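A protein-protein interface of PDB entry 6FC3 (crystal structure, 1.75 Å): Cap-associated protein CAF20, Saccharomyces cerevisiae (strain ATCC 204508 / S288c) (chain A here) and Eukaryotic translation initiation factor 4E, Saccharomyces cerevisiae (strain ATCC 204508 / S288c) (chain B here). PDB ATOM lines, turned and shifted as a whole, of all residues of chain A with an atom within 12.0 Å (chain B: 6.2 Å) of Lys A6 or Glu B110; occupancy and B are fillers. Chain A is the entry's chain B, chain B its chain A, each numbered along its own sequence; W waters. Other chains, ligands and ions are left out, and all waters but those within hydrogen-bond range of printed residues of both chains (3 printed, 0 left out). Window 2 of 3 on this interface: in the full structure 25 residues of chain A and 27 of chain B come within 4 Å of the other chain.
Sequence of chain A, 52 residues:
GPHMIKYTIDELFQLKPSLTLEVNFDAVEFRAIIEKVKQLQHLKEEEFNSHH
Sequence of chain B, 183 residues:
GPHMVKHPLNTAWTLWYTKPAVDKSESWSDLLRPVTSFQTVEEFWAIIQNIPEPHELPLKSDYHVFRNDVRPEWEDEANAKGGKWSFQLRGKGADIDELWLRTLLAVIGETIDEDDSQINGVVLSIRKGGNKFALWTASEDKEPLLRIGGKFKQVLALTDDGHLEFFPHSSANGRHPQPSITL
The backbone carbonyl oxygen of Glu B110 lies within hydrogen-bond range of the side-chain amino group of Lys A6, at 2.7 Å.
The side-chain amide oxygen of Asn B10 sits at hydrogen-bond distance from the backbone NH of Ile A5 (3.4 Å).
The backbone carbonyl oxygen (O) of Gly B109 sits at hydrogen-bond distance from the backbone NH (N) of Tyr A7.
The backbone carbonyl oxygen (O) of Ala B106 lies within hydrogen-bond range of the backbone NH (N) of Ile B112 (3.4 Å).
The backbone NH of Thr B111 sits at hydrogen-bond distance from the backbone carbonyl oxygen of Ala B106 (3.1 Å).
The side-chain amide nitrogen (ND2) of Asn B10 is in hydrogen-bond range of the side-chain carboxylate (OE2) of Glu B110 (3.1 Å).
The guanidinium group of Arg B67 is in salt-bridge range of the side-chain carboxylate of Glu B110, 2.7 Å away.
Asn B10 touches His A3.
Met A4 touches Asn B10.
Met A4 touches Glu B110 (SD to CB, 3.7 Å).
Ile A5 touches Glu B110 (O to CG, 3.7 Å).
Gly B109 touches Lys A6.
Thr B111 touches Tyr A7 (CG2 to O, 3.4 Å).
Ile A9 touches Ala B106 (CG1 to N, 3.97 Å).
Leu A12 touches Leu B105.
Leu B105 touches Phe A13.
Of the printed residues of chain B, His A3 touches Asn B10 (3.8 Å).
Of chain B, only Gly B109 (3.2 Å) and Glu B110 (2.7 Å) come within 4 Å of Lys A6.
Of the printed residues of chain B, Phe A13 touches Leu B105.
Of chain A, only His A3, Met A4 and Ile A5 come within 4 Å of Asn B10.
No residue of chain A comes within 4 Å of Thr B11.
Printed residues of chain A within 4 Å of Leu B105: Leu A12 (3.5 Å) and Phe A13 (3.6 Å).
Ala B106 touches one residue of chain A.
No residue of chain A comes within 4 Å of Val B107.
Ile B108 touches none of the printed residues of chain A.
Gly B109 touches two residues of chain A.
Glu B110 touches three residues of chain A.
Thr B111 touches one residue of chain A.
No residue of chain A comes within 4 Å of Ile B112.
No residue of chain A comes within 4 Å of Ile B119.
The nearest residue of chain B that does not touch Lys A6 is Asp B113 (4.4 Å).
The nearest residue of chain A that does not touch Glu B110 is Tyr A7 (4.9 Å).
The nearest printed residue of chain B that does not touch Ile A5 is Gly B109 (4.1 Å).
Of the 16 printed residues of chain B, 6 touch a printed residue of chain A.
Printed residues of chain B that touch a printed residue of chain A: Asn B10, Leu B105, Ala B106, Gly B109, Glu B110 and Thr B111.
Hydrophobic or aromatic side chains of chain B within 4 Å of the printed part of chain A: Leu B105.
Hydrophobic or aromatic side chains of chain A within 4 Å of the printed part of chain B: His A3, Met A4, Ile A9, Leu A12 and Phe A13.
Among the printed residues, 12 pairs touch across the chains.
Among the printed residues, no Asp or Glu carboxylate lies within 4 Å of a Lys or Arg side-chain nitrogen of the other chain.
Water W3 lies within hydrogen-bond range of the backbone carbonyl oxygen of Tyr A7 (2.5 Å), the side-chain hydroxyl of Thr B111 (2.8 Å) and the backbone carbonyl oxygen of Leu B105 (2.8 Å).
Water W1 bridges O of His A3 (2.7 Å) and ND2 of Asn B10 (3.4 Å).
Water W2 lies within hydrogen-bond range of O of Ile A5, N of Asn B10 and O of Ile B108.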
ATOM      1  N   PRO A   2      23.384 -20.490  21.311  1.00  0.00           N
ATOM      2  CA  PRO A   2      21.964 -20.418  20.956  1.00  0.00           C
ATOM      3  C   PRO A   2      21.218 -21.736  21.161  1.00  0.00           C
ATOM      4  O   PRO A   2      21.790 -22.836  21.190  1.00  0.00           O
ATOM      5  CB  PRO A   2      21.985 -20.032  19.471  1.00  0.00           C
ATOM      6  CG  PRO A   2      23.336 -19.520  19.193  1.00  0.00           C
ATOM      7  CD  PRO A   2      24.265 -20.180  20.171  1.00  0.00           C
ATOM      8  N   HIS A   3      19.900 -21.601  21.274  1.00  0.00           N
ATOM      9  CA  HIS A   3      18.991 -22.740  21.301  1.00  0.00           C
ATOM     10  C   HIS A   3      17.641 -22.296  20.769  1.00  0.00           C
ATOM     11  O   HIS A   3      17.212 -21.164  21.027  1.00  0.00           O
ATOM     12  CB  HIS A   3      18.860 -23.307  22.718  1.00  0.00           C
ATOM     13  CG  HIS A   3      18.070 -22.432  23.641  1.00  0.00           C
ATOM     14  ND1 HIS A   3      18.645 -21.438  24.402  1.00  0.00           N
ATOM     15  CD2 HIS A   3      16.742 -22.386  23.901  1.00  0.00           C
ATOM     16  CE1 HIS A   3      17.706 -20.826  25.102  1.00  0.00           C
ATOM     17  NE2 HIS A   3      16.544 -21.383  24.817  1.00  0.00           N
ATOM     18  N   MET A   4      16.967 -23.189  20.028  1.00  0.00           N
ATOM     19  CA  MET A   4      15.708 -22.833  19.372  1.00  0.00           C
ATOM     20  C   MET A   4      14.973 -24.073  18.887  1.00  0.00           C
ATOM     21  O   MET A   4      15.594 -25.031  18.419  1.00  0.00           O
ATOM     22  CB  MET A   4      15.978 -21.894  18.186  1.00  0.00           C
ATOM     23  CG  MET A   4      14.758 -21.473  17.370  1.00  0.00           C
ATOM     24  SD  MET A   4      13.456 -20.661  18.318  1.00  0.00           S
ATOM     25  CE  MET A   4      14.366 -19.339  19.091  1.00  0.00           C
ATOM     26  N   ILE A   5      13.644 -24.060  19.017  1.00  0.00           N
ATOM     27  CA  ILE A   5      12.781 -24.988  18.293  1.00  0.00           C
ATOM     28  C   ILE A   5      11.729 -24.175  17.578  1.00  0.00           C
ATOM     29  O   ILE A   5      11.037 -23.375  18.215  1.00  0.00           O
ATOM     30  CB  ILE A   5      12.068 -26.014  19.194  1.00  0.00           C
ATOM     31  CG1 ILE A   5      13.005 -26.713  20.143  1.00  0.00           C
ATOM     32  CG2 ILE A   5      11.328 -27.019  18.275  1.00  0.00           C
ATOM     33  CD1 ILE A   5      12.246 -27.613  21.109  1.00  0.00           C
ATOM     34  N   LYS A   6      11.592 -24.398  16.260  1.00  0.00           N
ATOM     35  CA  LYS A   6      10.607 -23.727  15.428  1.00  0.00           C
ATOM     36  C   LYS A   6       9.618 -24.744  14.863  1.00  0.00           C
ATOM     37  O   LYS A   6       9.995 -25.857  14.500  1.00  0.00           O
ATOM     38  CB  LYS A   6      11.254 -22.967  14.274  1.00  0.00           C
ATOM     39  CG  LYS A   6      12.095 -21.792  14.715  1.00  0.00           C
ATOM     40  CD  LYS A   6      12.631 -21.042  13.520  1.00  0.00           C
ATOM     41  CE  LYS A   6      13.602 -19.936  13.911  1.00  0.00           C
ATOM     42  NZ  LYS A   6      12.945 -18.914  14.766  1.00  0.00           N
ATOM     43  N   TYR A   7       8.348 -24.356  14.813  1.00  0.00           N
ATOM     44  CA  TYR A   7       7.279 -25.123  14.184  1.00  0.00           C
ATOM     45  C   TYR A   7       6.540 -24.199  13.235  1.00  0.00           C
ATOM     46  O   TYR A   7       6.194 -23.074  13.616  1.00  0.00           O
ATOM     47  CB  TYR A   7       6.260 -25.655  15.198  1.00  0.00           C
ATOM     48  CG  TYR A   7       6.726 -26.632  16.229  1.00  0.00           C
ATOM     49  CD1 TYR A   7       7.287 -26.192  17.435  1.00  0.00           C
ATOM     50  CD2 TYR A   7       6.586 -27.988  16.029  1.00  0.00           C
ATOM     51  CE1 TYR A   7       7.696 -27.073  18.390  1.00  0.00           C
ATOM     52  CE2 TYR A   7       6.981 -28.897  16.998  1.00  0.00           C
ATOM     53  CZ  TYR A   7       7.556 -28.438  18.169  1.00  0.00           C
ATOM     54  OH  TYR A   7       7.946 -29.350  19.117  1.00  0.00           O
ATOM     55  N   THR A   8       6.282 -24.651  12.011  1.00  0.00           N
ATOM     56  CA  THR A   8       5.471 -23.820  11.142  1.00  0.00           C
ATOM     57  C   THR A   8       4.016 -23.845  11.597  1.00  0.00           C
ATOM     58  O   THR A   8       3.575 -24.740  12.320  1.00  0.00           O
ATOM     59  CB  THR A   8       5.538 -24.291   9.699  1.00  0.00           C
ATOM     60  OG1 THR A   8       4.937 -25.591   9.623  1.00  0.00           O
ATOM     61  CG2 THR A   8       6.984 -24.338   9.224  1.00  0.00           C
ATOM     62  N   ILE A   9       3.252 -22.889  11.102  1.00  0.00           N
ATOM     63  CA  ILE A   9       1.825 -22.857  11.405  1.00  0.00           C
ATOM     64  C   ILE A   9       1.177 -24.161  10.965  1.00  0.00           C
ATOM     65  O   ILE A   9       0.440 -24.795  11.728  1.00  0.00           O
ATOM     66  CB  ILE A   9       1.173 -21.623  10.755  1.00  0.00           C
ATOM     67  CG1 ILE A   9       1.589 -20.348  11.526  1.00  0.00           C
ATOM     68  CG2 ILE A   9      -0.363 -21.742  10.714  1.00  0.00           C
ATOM     69  CD1 ILE A   9       1.393 -19.072  10.764  1.00  0.00           C
ATOM     70  N   ASP A  10       1.468 -24.599   9.732  1.00  0.00           N
ATOM     71  CA  ASP A  10       0.883 -25.848   9.242  1.00  0.00           C
ATOM     72  C   ASP A  10       1.285 -27.028  10.113  1.00  0.00           C
ATOM     73  O   ASP A  10       0.481 -27.940  10.349  1.00  0.00           O
ATOM     74  CB  ASP A  10       1.306 -26.098   7.794  1.00  0.00           C
ATOM     75  CG  ASP A  10       0.630 -25.151   6.825  1.00  0.00           C
ATOM     76  OD1 ASP A  10      -0.416 -24.586   7.204  1.00  0.00           O
ATOM     77  OD2 ASP A  10       1.143 -24.973   5.695  1.00  0.00           O
ATOM     78  N   GLU A  11       2.546 -27.069  10.548  1.00  0.00           N
ATOM     79  CA  GLU A  11       2.988 -28.147  11.430  1.00  0.00           C
ATOM     80  C   GLU A  11       2.151 -28.176  12.690  1.00  0.00           C
ATOM     81  O   GLU A  11       1.737 -29.248  13.154  1.00  0.00           O
ATOM     82  CB  GLU A  11       4.459 -27.948  11.807  1.00  0.00           C
ATOM     83  CG  GLU A  11       5.448 -28.962  11.414  1.00  0.00           C
ATOM     84  CD  GLU A  11       6.830 -28.571  11.955  1.00  0.00           C
ATOM     85  OE1 GLU A  11       7.219 -27.397  11.748  1.00  0.00           O
ATOM     86  OE2 GLU A  11       7.480 -29.400  12.624  1.00  0.00           O
ATOM     87  N   LEU A  12       1.911 -27.000  13.272  1.00  0.00           N
ATOM     88  CA  LEU A  12       1.181 -26.923  14.530  1.00  0.00           C
ATOM     89  C   LEU A  12      -0.279 -27.321  14.344  1.00  0.00           C
ATOM     90  O   LEU A  12      -0.853 -28.034  15.183  1.00  0.00           O
ATOM     91  CB  LEU A  12       1.309 -25.512  15.096  1.00  0.00           C
ATOM     92  CG  LEU A  12       2.733 -25.237  15.594  1.00  0.00           C
ATOM     93  CD1 LEU A  12       2.910 -23.787  15.846  1.00  0.00           C
ATOM     94  CD2 LEU A  12       3.035 -25.952  16.859  1.00  0.00           C
ATOM     95  N   PHE A  13      -0.881 -26.924  13.226  1.00  0.00           N
ATOM     96  CA  PHE A  13      -2.241 -27.378  12.932  1.00  0.00           C
ATOM     97  C   PHE A  13      -2.302 -28.887  12.754  1.00  0.00           C
ATOM     98  O   PHE A  13      -3.290 -29.520  13.139  1.00  0.00           O
ATOM     99  CB  PHE A  13      -2.779 -26.721  11.661  1.00  0.00           C
ATOM    100  CG  PHE A  13      -3.410 -25.394  11.876  1.00  0.00           C
ATOM    101  CD1 PHE A  13      -4.520 -25.267  12.691  1.00  0.00           C
ATOM    102  CD2 PHE A  13      -2.931 -24.281  11.210  1.00  0.00           C
ATOM    103  CE1 PHE A  13      -5.120 -24.039  12.862  1.00  0.00           C
ATOM    104  CE2 PHE A  13      -3.537 -23.069  11.365  1.00  0.00           C
ATOM    105  CZ  PHE A  13      -4.629 -22.943  12.205  1.00  0.00           C
ATOM    106  N   GLN A  14      -1.289 -29.478  12.118  1.00  0.00           N
ATOM    107  CA  GLN A  14      -1.290 -30.927  11.926  1.00  0.00           C
ATOM    108  C   GLN A  14      -1.235 -31.671  13.251  1.00  0.00           C
ATOM    109  O   GLN A  14      -1.613 -32.848  13.306  1.00  0.00           O
ATOM    110  CB  GLN A  14      -0.107 -31.371  11.068  1.00  0.00           C
ATOM    111  CG  GLN A  14      -0.146 -30.906   9.634  1.00  0.00           C
ATOM    112  CD  GLN A  14       1.213 -31.024   8.943  1.00  0.00           C
ATOM    113  OE1 GLN A  14       2.170 -31.565   9.504  1.00  0.00           O
ATOM    114  NE2 GLN A  14       1.302 -30.508   7.722  1.00  0.00           N
ATOM    115  N   LEU A  15      -0.786 -31.010  14.313  1.00  0.00           N
ATOM    116  CA  LEU A  15      -0.732 -31.604  15.642  1.00  0.00           C
ATOM    117  C   LEU A  15      -1.988 -31.323  16.476  1.00  0.00           C
ATOM    118  O   LEU A  15      -2.054 -31.754  17.635  1.00  0.00           O
ATOM    119  CB  LEU A  15       0.527 -31.112  16.367  1.00  0.00           C
ATOM    120  CG  LEU A  15       1.846 -31.641  15.794  1.00  0.00           C
ATOM    121  CD1 LEU A  15       3.065 -30.813  16.162  1.00  0.00           C
ATOM    122  CD2 LEU A  15       2.057 -33.071  16.253  1.00  0.00           C
ATOM    123  N   ASN B  10       9.642 -24.008  22.165  1.00  0.00           N
ATOM    124  CA  ASN B  10      10.898 -23.347  22.511  1.00  0.00           C
ATOM    125  C   ASN B  10      10.882 -22.810  23.947  1.00  0.00           C
ATOM    126  O   ASN B  10      11.865 -22.952  24.676  1.00  0.00           O
ATOM    127  CB  ASN B  10      11.180 -22.217  21.537  1.00  0.00           C
ATOM    128  CG  ASN B  10      12.491 -21.516  21.822  1.00  0.00           C
ATOM    129  OD1 ASN B  10      13.538 -22.145  21.865  1.00  0.00           O
ATOM    130  ND2 ASN B  10      12.440 -20.215  22.006  1.00  0.00           N
ATOM    131  N   THR B  11       9.805 -22.153  24.365  1.00  0.00           N
ATOM    132  CA  THR B  11       9.718 -21.724  25.757  1.00  0.00           C
ATOM    133  C   THR B  11       8.330 -22.046  26.272  1.00  0.00           C
ATOM    134  O   THR B  11       7.423 -22.349  25.498  1.00  0.00           O
ATOM    135  CB  THR B  11       9.957 -20.212  25.985  1.00  0.00           C
ATOM    136  OG1 THR B  11       8.928 -19.439  25.336  1.00  0.00           O
ATOM    137  CG2 THR B  11      11.299 -19.776  25.482  1.00  0.00           C
ATOM    138  N   TRP B  13       4.827 -20.708  27.983  1.00  0.00           N
ATOM    139  CA  TRP B  13       3.986 -19.531  27.843  1.00  0.00           C
ATOM    140  C   TRP B  13       2.884 -19.576  28.890  1.00  0.00           C
ATOM    141  O   TRP B  13       2.493 -20.649  29.352  1.00  0.00           O
ATOM    142  CB  TRP B  13       3.337 -19.453  26.439  1.00  0.00           C
ATOM    143  CG  TRP B  13       4.340 -19.387  25.350  1.00  0.00           C
ATOM    144  CD1 TRP B  13       5.053 -20.435  24.854  1.00  0.00           C
ATOM    145  CD2 TRP B  13       4.769 -18.232  24.643  1.00  0.00           C
ATOM    146  NE1 TRP B  13       5.906 -20.003  23.883  1.00  0.00           N
ATOM    147  CE2 TRP B  13       5.751 -18.653  23.725  1.00  0.00           C
ATOM    148  CE3 TRP B  13       4.426 -16.876  24.693  1.00  0.00           C
ATOM    149  CZ2 TRP B  13       6.406 -17.783  22.890  1.00  0.00           C
ATOM    150  CZ3 TRP B  13       5.064 -16.011  23.845  1.00  0.00           C
ATOM    151  CH2 TRP B  13       6.043 -16.463  22.949  1.00  0.00           C
ATOM    152  N   ARG B  67       5.598 -15.060  27.333  1.00  0.00           N
ATOM    153  CA  ARG B  67       6.629 -15.973  27.802  1.00  0.00           C
ATOM    154  C   ARG B  67       6.646 -15.984  29.329  1.00  0.00           C
ATOM    155  O   ARG B  67       6.368 -14.971  29.979  1.00  0.00           O
ATOM    156  CB  ARG B  67       8.002 -15.577  27.248  1.00  0.00           C
ATOM    157  CG  ARG B  67       8.115 -15.692  25.755  1.00  0.00           C
ATOM    158  CD  ARG B  67       9.540 -15.494  25.316  1.00  0.00           C
ATOM    159  NE  ARG B  67       9.610 -15.169  23.899  1.00  0.00           N
ATOM    160  CZ  ARG B  67       9.731 -16.052  22.912  1.00  0.00           C
ATOM    161  NH1 ARG B  67       9.799 -17.353  23.169  1.00  0.00           N
ATOM    162  NH2 ARG B  67       9.781 -15.621  21.657  1.00  0.00           N
ATOM    163  N   LEU B 105      -0.023 -19.273  16.824  1.00  0.00           N
ATOM    164  CA  LEU B 105       0.829 -20.318  16.276  1.00  0.00           C
ATOM    165  C   LEU B 105       2.129 -19.739  15.733  1.00  0.00           C
ATOM    166  O   LEU B 105       3.203 -20.328  15.914  1.00  0.00           O
ATOM    167  CB  LEU B 105       0.088 -21.095  15.192  1.00  0.00           C
ATOM    168  CG  LEU B 105      -1.194 -21.826  15.637  1.00  0.00           C
ATOM    169  CD1 LEU B 105      -1.822 -22.551  14.448  1.00  0.00           C
ATOM    170  CD2 LEU B 105      -0.927 -22.781  16.758  1.00  0.00           C
ATOM    171  N   ALA B 106       2.048 -18.597  15.055  1.00  0.00           N
ATOM    172  CA  ALA B 106       3.264 -17.929  14.584  1.00  0.00           C
ATOM    173  C   ALA B 106       4.177 -17.557  15.736  1.00  0.00           C
ATOM    174  O   ALA B 106       5.397 -17.600  15.589  1.00  0.00           O
ATOM    175  CB  ALA B 106       2.906 -16.689  13.767  1.00  0.00           C
ATOM    176  N   VAL B 107       3.614 -17.201  16.885  1.00  0.00           N
ATOM    177  CA  VAL B 107       4.407 -16.768  18.026  1.00  0.00           C
ATOM    178  C   VAL B 107       4.995 -17.954  18.780  1.00  0.00           C
ATOM    179  O   VAL B 107       6.209 -18.009  19.028  1.00  0.00           O
ATOM    180  CB  VAL B 107       3.535 -15.892  18.948  1.00  0.00           C
ATOM    181  CG1 VAL B 107       4.204 -15.688  20.293  1.00  0.00           C
ATOM    182  CG2 VAL B 107       3.239 -14.548  18.275  1.00  0.00           C
ATOM    183  N   ILE B 108       4.166 -18.918  19.172  1.00  0.00           N
ATOM    184  CA  ILE B 108       4.717 -20.011  19.969  1.00  0.00           C
ATOM    185  C   ILE B 108       5.588 -20.922  19.120  1.00  0.00           C
ATOM    186  O   ILE B 108       6.470 -21.608  19.646  1.00  0.00           O
ATOM    187  CB  ILE B 108       3.625 -20.824  20.674  1.00  0.00           C
ATOM    188  CG1 ILE B 108       2.829 -21.634  19.655  1.00  0.00           C
ATOM    189  CG2 ILE B 108       2.751 -19.877  21.528  1.00  0.00           C
ATOM    190  CD1 ILE B 108       1.767 -22.583  20.259  1.00  0.00           C
ATOM    191  N   GLY B 109       5.379 -20.925  17.814  1.00  0.00           N
ATOM    192  CA  GLY B 109       6.189 -21.707  16.913  1.00  0.00           C
ATOM    193  C   GLY B 109       7.447 -20.990  16.479  1.00  0.00           C
ATOM    194  O   GLY B 109       8.270 -21.585  15.788  1.00  0.00           O
ATOM    195  N   GLU B 110       7.569 -19.714  16.862  1.00  0.00           N
ATOM    196  CA  GLU B 110       8.786 -18.911  16.748  1.00  0.00           C
ATOM    197  C   GLU B 110       9.117 -18.566  15.302  1.00  0.00           C
ATOM    198  O   GLU B 110      10.277 -18.303  14.980  1.00  0.00           O
ATOM    199  CB  GLU B 110       9.988 -19.598  17.418  1.00  0.00           C
ATOM    200  CG  GLU B 110       9.723 -19.994  18.884  1.00  0.00           C
ATOM    201  CD  GLU B 110       9.809 -18.833  19.884  1.00  0.00           C
ATOM    202  OE1 GLU B 110      10.042 -17.683  19.474  1.00  0.00           O
ATOM    203  OE2 GLU B 110       9.678 -19.070  21.103  1.00  0.00           O
ATOM    204  N   THR B 111       8.128 -18.540  14.404  1.00  0.00           N
ATOM    205  CA  THR B 111       8.423 -18.204  13.024  1.00  0.00           C
ATOM    206  C   THR B 111       8.191 -16.730  12.700  1.00  0.00           C
ATOM    207  O   THR B 111       8.559 -16.294  11.612  1.00  0.00           O
ATOM    208  CB  THR B 111       7.610 -19.078  12.064  1.00  0.00           C
ATOM    209  OG1 THR B 111       6.221 -18.895  12.300  1.00  0.00           O
ATOM    210  CG2 THR B 111       8.020 -20.555  12.214  1.00  0.00           C
ATOM    211  N   ILE B 112       7.604 -15.960  13.606  1.00  0.00           N
ATOM    212  CA  ILE B 112       7.434 -14.540  13.347  1.00  0.00           C
ATOM    213  C   ILE B 112       8.717 -13.790  13.683  1.00  0.00           C
ATOM    214  O   ILE B 112       8.951 -12.688  13.164  1.00  0.00           O
ATOM    215  CB  ILE B 112       6.197 -14.066  14.139  1.00  0.00           C
ATOM    216  CG1 ILE B 112       5.505 -12.902  13.439  1.00  0.00           C
ATOM    217  CG2 ILE B 112       6.553 -13.717  15.589  1.00  0.00           C
ATOM    218  CD1 ILE B 112       4.163 -12.650  13.975  1.00  0.00           C
ATOM    219  N   ASP B 113       9.598 -14.421  14.448  1.00  0.00           N
ATOM    220  CA  ASP B 113      10.620 -13.766  15.251  1.00  0.00           C
ATOM    221  C   ASP B 113      11.985 -13.790  14.573  1.00  0.00           C
ATOM    222  O   ASP B 113      12.286 -14.665  13.756  1.00  0.00           O
ATOM    223  CB  ASP B 113      10.698 -14.473  16.610  1.00  0.00           C
ATOM    224  CG  ASP B 113      10.982 -13.527  17.750  1.00  0.00           C
ATOM    225  OD1 ASP B 113      11.526 -12.430  17.489  1.00  0.00           O
ATOM    226  OD2 ASP B 113      10.657 -13.888  18.906  1.00  0.00           O
ATOM    227  N   GLU B 114      12.818 -12.808  14.940  1.00  0.00           N
ATOM    228  CA  GLU B 114      14.210 -12.764  14.520  1.00  0.00           C
ATOM    229  C   GLU B 114      15.028 -13.848  15.221  1.00  0.00           C
ATOM    230  O   GLU B 114      16.263 -13.838  15.165  1.00  0.00           O
ATOM    231  CB  GLU B 114      14.792 -11.382  14.817  1.00  0.00           C
ATOM    232  CG  GLU B 114      13.988 -10.240  14.187  1.00  0.00           C
ATOM    233  CD  GLU B 114      14.319 -10.026  12.716  1.00  0.00           C
ATOM    234  OE1 GLU B 114      15.421  -9.525  12.427  1.00  0.00           O
ATOM    235  OE2 GLU B 114      13.490 -10.373  11.849  1.00  0.00           O
ATOM    236  N   GLN B 118      13.150  -9.555  19.862  1.00  0.00           N
ATOM    237  CA  GLN B 118      12.477 -10.807  20.142  1.00  0.00           C
ATOM    238  C   GLN B 118      11.025 -10.492  20.491  1.00  0.00           C
ATOM    239  O   GLN B 118      10.675  -9.355  20.780  1.00  0.00           O
ATOM    240  CB  GLN B 118      13.153 -11.570  21.282  1.00  0.00           C
ATOM    241  CG  GLN B 118      14.444 -12.287  20.887  1.00  0.00           C
ATOM    242  CD  GLN B 118      14.204 -13.463  19.947  1.00  0.00           C
ATOM    243  OE1 GLN B 118      14.352 -13.338  18.729  1.00  0.00           O
ATOM    244  NE2 GLN B 118      13.846 -14.616  20.511  1.00  0.00           N
ATOM    245  N   ILE B 119      10.195 -11.510  20.429  1.00  0.00           N
ATOM    246  CA  ILE B 119       8.762 -11.390  20.665  1.00  0.00           C
ATOM    247  C   ILE B 119       8.481 -11.810  22.109  1.00  0.00           C
ATOM    248  O   ILE B 119       8.786 -12.941  22.497  1.00  0.00           O
ATOM    249  CB  ILE B 119       7.985 -12.261  19.669  1.00  0.00           C
ATOM    250  CG1 ILE B 119       8.218 -11.780  18.237  1.00  0.00           C
ATOM    251  CG2 ILE B 119       6.501 -12.279  19.990  1.00  0.00           C
ATOM    252  CD1 ILE B 119       7.554 -10.494  17.913  1.00  0.00           C
HETATM  253  O   HOH W   1      15.687 -19.526  22.498  1.00  0.00           O
HETATM  254  O   HOH W   2       8.545 -23.625  19.559  1.00  0.00           O
HETATM  255  O   HOH W   3       4.919 -20.870  13.709  1.00  0.00           O
